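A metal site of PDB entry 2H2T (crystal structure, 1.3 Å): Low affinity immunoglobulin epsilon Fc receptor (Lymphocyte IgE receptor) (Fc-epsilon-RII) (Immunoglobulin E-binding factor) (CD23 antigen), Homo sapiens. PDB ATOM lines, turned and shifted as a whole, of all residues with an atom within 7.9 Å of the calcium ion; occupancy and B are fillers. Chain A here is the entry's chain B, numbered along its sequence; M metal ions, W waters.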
ATOM      1  N   PHE A  86      14.975  23.769 -13.781  1.00  0.00           N
ATOM      2  CA  PHE A  86      15.599  25.078 -13.681  1.00  0.00           C
ATOM      3  C   PHE A  86      14.546  26.184 -13.871  1.00  0.00           C
ATOM      4  O   PHE A  86      13.850  26.200 -14.882  1.00  0.00           O
ATOM      5  CB  PHE A  86      16.716  25.207 -14.724  1.00  0.00           C
ATOM      6  CG  PHE A  86      17.942  24.463 -14.385  1.00  0.00           C
ATOM      7  CD1 PHE A  86      18.192  23.208 -14.956  1.00  0.00           C
ATOM      8  CD2 PHE A  86      18.860  24.976 -13.529  1.00  0.00           C
ATOM      9  CE1 PHE A  86      19.319  22.520 -14.636  1.00  0.00           C
ATOM     10  CE2 PHE A  86      19.993  24.265 -13.206  1.00  0.00           C
ATOM     11  CZ  PHE A  86      20.207  23.032 -13.762  1.00  0.00           C
ATOM     12  N   TRP A  99      22.275  27.330 -23.083  1.00  0.00           N
ATOM     13  CA  TRP A  99      23.226  26.386 -22.516  1.00  0.00           C
ATOM     14  C   TRP A  99      24.434  26.195 -23.395  1.00  0.00           C
ATOM     15  O   TRP A  99      24.315  26.077 -24.605  1.00  0.00           O
ATOM     16  CB  TRP A  99      22.560  25.026 -22.326  1.00  0.00           C
ATOM     17  CG  TRP A  99      21.418  25.028 -21.369  1.00  0.00           C
ATOM     18  CD1 TRP A  99      20.085  24.852 -21.668  1.00  0.00           C
ATOM     19  CD2 TRP A  99      21.474  25.198 -19.937  1.00  0.00           C
ATOM     20  NE1 TRP A  99      19.338  24.929 -20.547  1.00  0.00           N
ATOM     21  CE2 TRP A  99      20.160  25.117 -19.459  1.00  0.00           C
ATOM     22  CE3 TRP A  99      22.508  25.397 -19.024  1.00  0.00           C
ATOM     23  CZ2 TRP A  99      19.855  25.218 -18.129  1.00  0.00           C
ATOM     24  CZ3 TRP A  99      22.204  25.479 -17.684  1.00  0.00           C
ATOM     25  CH2 TRP A  99      20.891  25.394 -17.256  1.00  0.00           C
ATOM     26  N   GLY A 102      26.667  20.392 -23.996  1.00  0.00           N
ATOM     27  CA  GLY A 102      26.786  19.428 -22.920  1.00  0.00           C
ATOM     28  C   GLY A 102      26.076  19.848 -21.644  1.00  0.00           C
ATOM     29  O   GLY A 102      25.929  19.043 -20.719  1.00  0.00           O
ATOM     30  N   GLU A 103      25.635  21.117 -21.549  1.00  0.00           N
ATOM     31  CA  GLU A 103      24.978  21.599 -20.321  1.00  0.00           C
ATOM     32  C   GLU A 103      23.447  21.614 -20.500  1.00  0.00           C
ATOM     33  O   GLU A 103      22.944  21.751 -21.623  1.00  0.00           O
ATOM     34  CB  GLU A 103      25.423  23.021 -20.020  1.00  0.00           C
ATOM     35  CG  GLU A 103      26.933  23.180 -19.933  1.00  0.00           C
ATOM     36  CD  GLU A 103      27.533  22.529 -18.741  1.00  0.00           C
ATOM     37  OE1 GLU A 103      26.822  22.297 -17.756  1.00  0.00           O
ATOM     38  OE2 GLU A 103      28.756  22.213 -18.812  1.00  0.00           O
ATOM     39  N   PRO A 104      22.711  21.501 -19.407  1.00  0.00           N
ATOM     40  CA  PRO A 104      23.192  21.339 -18.061  1.00  0.00           C
ATOM     41  C   PRO A 104      23.656  19.927 -17.798  1.00  0.00           C
ATOM     42  O   PRO A 104      23.062  18.951 -18.316  1.00  0.00           O
ATOM     43  CB  PRO A 104      21.947  21.651 -17.191  1.00  0.00           C
ATOM     44  CG  PRO A 104      20.789  21.256 -18.051  1.00  0.00           C
ATOM     45  CD  PRO A 104      21.237  21.553 -19.459  1.00  0.00           C
ATOM     46  N   THR A 105      24.684  19.796 -16.998  1.00  0.00           N
ATOM     47  CA  THR A 105      25.182  18.466 -16.674  1.00  0.00           C
ATOM     48  C   THR A 105      24.386  17.771 -15.509  1.00  0.00           C
ATOM     49  O   THR A 105      24.227  16.519 -15.493  1.00  0.00           O
ATOM     50  CB  THR A 105      26.690  18.519 -16.426  1.00  0.00           C
ATOM     51  OG1 THR A 105      27.000  19.587 -15.533  1.00  0.00           O
ATOM     52  CG2 THR A 105      27.463  18.749 -17.754  1.00  0.00           C
ATOM     53  N   SER A 106      23.830  18.585 -14.607  1.00  0.00           N
ATOM     54  CA  SER A 106      23.028  18.090 -13.470  1.00  0.00           C
ATOM     55  C   SER A 106      22.042  17.025 -13.901  1.00  0.00           C
ATOM     56  O   SER A 106      21.194  17.257 -14.746  1.00  0.00           O
ATOM     57  CB  SER A 106      22.285  19.238 -12.781  1.00  0.00           C
ATOM     58  OG  SER A 106      21.541  20.007 -13.710  1.00  0.00           O
ATOM     59  N   ASP A 112      21.129  22.603  -9.525  1.00  0.00           N
ATOM     60  CA  ASP A 112      22.224  23.421  -9.087  1.00  0.00           C
ATOM     61  C   ASP A 112      21.922  24.904  -9.431  1.00  0.00           C
ATOM     62  O   ASP A 112      20.786  25.319  -9.616  1.00  0.00           O
ATOM     63  CB  ASP A 112      23.529  23.039  -9.785  1.00  0.00           C
ATOM     64  CG  ASP A 112      23.858  21.634  -9.663  1.00  0.00           C
ATOM     65  OD1 ASP A 112      22.906  20.813  -9.583  1.00  0.00           O
ATOM     66  OD2 ASP A 112      25.108  21.324  -9.651  1.00  0.00           O
ATOM     67  N   CYS A 113      22.966  25.699  -9.458  1.00  0.00           N
ATOM     68  CA  CYS A 113      22.896  27.125  -9.713  1.00  0.00           C
ATOM     69  C   CYS A 113      23.530  27.414 -11.077  1.00  0.00           C
ATOM     70  O   CYS A 113      24.546  26.845 -11.431  1.00  0.00           O
ATOM     71  CB  CYS A 113      23.615  27.876  -8.577  1.00  0.00           C
ATOM     72  SG  CYS A 113      22.762  27.826  -7.027  1.00  0.00           S
ATOM     73  N   MET A 115      25.462  29.708 -13.993  1.00  0.00           N
ATOM     74  CA  MET A 115      26.366  30.793 -14.324  1.00  0.00           C
ATOM     75  C   MET A 115      26.451  30.991 -15.832  1.00  0.00           C
ATOM     76  O   MET A 115      26.144  30.078 -16.631  1.00  0.00           O
ATOM     77  CB  MET A 115      27.767  30.541 -13.768  1.00  0.00           C
ATOM     78  CG  MET A 115      28.442  29.301 -14.350  1.00  0.00           C
ATOM     79  SD  MET A 115      30.026  28.885 -13.673  1.00  0.00           S
ATOM     80  CE  MET A 115      31.005  30.136 -14.449  1.00  0.00           C
ATOM     81  N   ARG A 117      29.060  31.952 -18.748  1.00  0.00           N
ATOM     82  CA  ARG A 117      30.471  32.035 -19.132  1.00  0.00           C
ATOM     83  C   ARG A 117      30.741  33.334 -19.852  1.00  0.00           C
ATOM     84  O   ARG A 117      29.807  34.079 -20.223  1.00  0.00           O
ATOM     85  CB  ARG A 117      30.801  30.899 -20.107  1.00  0.00           C
ATOM     86  CG  ARG A 117      30.533  29.487 -19.647  1.00  0.00           C
ATOM     87  CD  ARG A 117      31.582  28.958 -18.719  1.00  0.00           C
ATOM     88  NE  ARG A 117      31.396  27.528 -18.457  1.00  0.00           N
ATOM     89  CZ  ARG A 117      31.972  26.920 -17.426  1.00  0.00           C
ATOM     90  NH1 ARG A 117      32.692  27.628 -16.572  1.00  0.00           N
ATOM     91  NH2 ARG A 117      31.807  25.623 -17.231  1.00  0.00           N
ATOM     92  N   TRP A 122      25.497  29.209 -20.853  1.00  0.00           N
ATOM     93  CA  TRP A 122      25.154  28.869 -19.495  1.00  0.00           C
ATOM     94  C   TRP A 122      25.745  27.524 -19.058  1.00  0.00           C
ATOM     95  O   TRP A 122      25.801  26.569 -19.855  1.00  0.00           O
ATOM     96  CB  TRP A 122      23.642  28.850 -19.311  1.00  0.00           C
ATOM     97  CG  TRP A 122      22.888  30.049 -19.776  1.00  0.00           C
ATOM     98  CD1 TRP A 122      23.372  31.261 -20.125  1.00  0.00           C
ATOM     99  CD2 TRP A 122      21.480  30.101 -19.980  1.00  0.00           C
ATOM    100  NE1 TRP A 122      22.335  32.097 -20.510  1.00  0.00           N
ATOM    101  CE2 TRP A 122      21.167  31.393 -20.419  1.00  0.00           C
ATOM    102  CE3 TRP A 122      20.433  29.172 -19.792  1.00  0.00           C
ATOM    103  CZ2 TRP A 122      19.874  31.774 -20.724  1.00  0.00           C
ATOM    104  CZ3 TRP A 122      19.151  29.572 -20.100  1.00  0.00           C
ATOM    105  CH2 TRP A 122      18.886  30.861 -20.556  1.00  0.00           C
ATOM    106  N   ASN A 123      26.108  27.475 -17.801  1.00  0.00           N
ATOM    107  CA  ASN A 123      26.569  26.276 -17.144  1.00  0.00           C
ATOM    108  C   ASN A 123      25.916  26.111 -15.765  1.00  0.00           C
ATOM    109  O   ASN A 123      25.944  27.047 -14.964  1.00  0.00           O
ATOM    110  CB  ASN A 123      28.105  26.367 -16.923  1.00  0.00           C
ATOM    111  CG  ASN A 123      28.638  25.266 -16.039  1.00  0.00           C
ATOM    112  OD1 ASN A 123      28.349  24.123 -16.267  1.00  0.00           O
ATOM    113  ND2 ASN A 123      29.460  25.616 -15.036  1.00  0.00           N
ATOM    114  N   ASP A 124      25.391  24.922 -15.444  1.00  0.00           N
ATOM    115  CA  ASP A 124      24.985  24.668 -14.082  1.00  0.00           C
ATOM    116  C   ASP A 124      26.227  24.337 -13.266  1.00  0.00           C
ATOM    117  O   ASP A 124      27.092  23.611 -13.712  1.00  0.00           O
ATOM    118  CB  ASP A 124      23.904  23.599 -13.966  1.00  0.00           C
ATOM    119  CG  ASP A 124      24.316  22.249 -14.520  1.00  0.00           C
ATOM    120  OD1 ASP A 124      23.620  21.275 -14.165  1.00  0.00           O
ATOM    121  OD2 ASP A 124      25.245  22.166 -15.373  1.00  0.00           O
ATOM    122  N   ALA A 125      26.292  24.838 -12.053  1.00  0.00           N
ATOM    123  CA  ALA A 125      27.512  24.797 -11.255  1.00  0.00           C
ATOM    124  C   ALA A 125      27.141  24.583  -9.796  1.00  0.00           C
ATOM    125  O   ALA A 125      25.983  24.779  -9.403  1.00  0.00           O
ATOM    126  CB  ALA A 125      28.279  26.142 -11.418  1.00  0.00           C
ATOM    127  N   PHE A 126      28.149  24.213  -8.993  1.00  0.00           N
ATOM    128  CA  PHE A 126      27.933  24.133  -7.546  1.00  0.00           C
ATOM    129  C   PHE A 126      27.577  25.509  -7.033  1.00  0.00           C
ATOM    130  O   PHE A 126      28.241  26.479  -7.356  1.00  0.00           O
ATOM    131  CB  PHE A 126      29.166  23.622  -6.815  1.00  0.00           C
ATOM    132  CG  PHE A 126      29.558  22.194  -7.183  1.00  0.00           C
ATOM    133  CD1 PHE A 126      30.380  21.933  -8.275  1.00  0.00           C
ATOM    134  CD2 PHE A 126      29.126  21.128  -6.419  1.00  0.00           C
ATOM    135  CE1 PHE A 126      30.755  20.619  -8.593  1.00  0.00           C
ATOM    136  CE2 PHE A 126      29.497  19.820  -6.744  1.00  0.00           C
ATOM    137  CZ  PHE A 126      30.307  19.586  -7.831  1.00  0.00           C
ATOM    138  N   ARG A 129      30.231  27.669  -5.421  1.00  0.00           N
ATOM    139  CA  ARG A 129      31.317  28.194  -6.225  1.00  0.00           C
ATOM    140  C   ARG A 129      31.428  29.733  -6.089  1.00  0.00           C
ATOM    141  O   ARG A 129      30.427  30.459  -6.073  1.00  0.00           O
ATOM    142  CB  ARG A 129      31.082  27.815  -7.675  1.00  0.00           C
ATOM    143  CG  ARG A 129      32.144  28.286  -8.628  1.00  0.00           C
ATOM    144  CD  ARG A 129      31.965  27.627  -9.961  1.00  0.00           C
ATOM    145  NE  ARG A 129      32.976  28.034 -10.916  1.00  0.00           N
ATOM    146  CZ  ARG A 129      33.253  27.385 -12.049  1.00  0.00           C
ATOM    147  NH1 ARG A 129      32.585  26.281 -12.366  1.00  0.00           N
ATOM    148  NH2 ARG A 129      34.194  27.845 -12.856  1.00  0.00           N
HETATM  149 CA    CA M   1      27.627  22.016 -15.450  1.00  0.00          CA
HETATM  150  O   HOH W   1      28.637  21.159 -13.541  1.00  0.00           O
HETATM  151  O   HOH W   2      29.671  21.381 -16.357  1.00  0.00           O
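The calcium ion is bound by water W1 (2.3 Å), water W2 (2.3 Å), OD1 of Asn 123 (2.4 Å), OD2 of Asp 124 (2.4 Å), O of Asp 124 (2.4 Å), OE1 of Glu 103 (2.5 Å) and OG1 of Thr 105 (2.5 Å).
The guanidinium group (NH2) of Arg 117 sits close to the side-chain amide nitrogen (ND2) of Asn 123. N of Asn 123 is in hydrogen-bond range of O of Met 115, at 2.9 Å. OD1 of Asp 124 is in hydrogen-bond range of OG of Ser 106 (2.5 Å).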
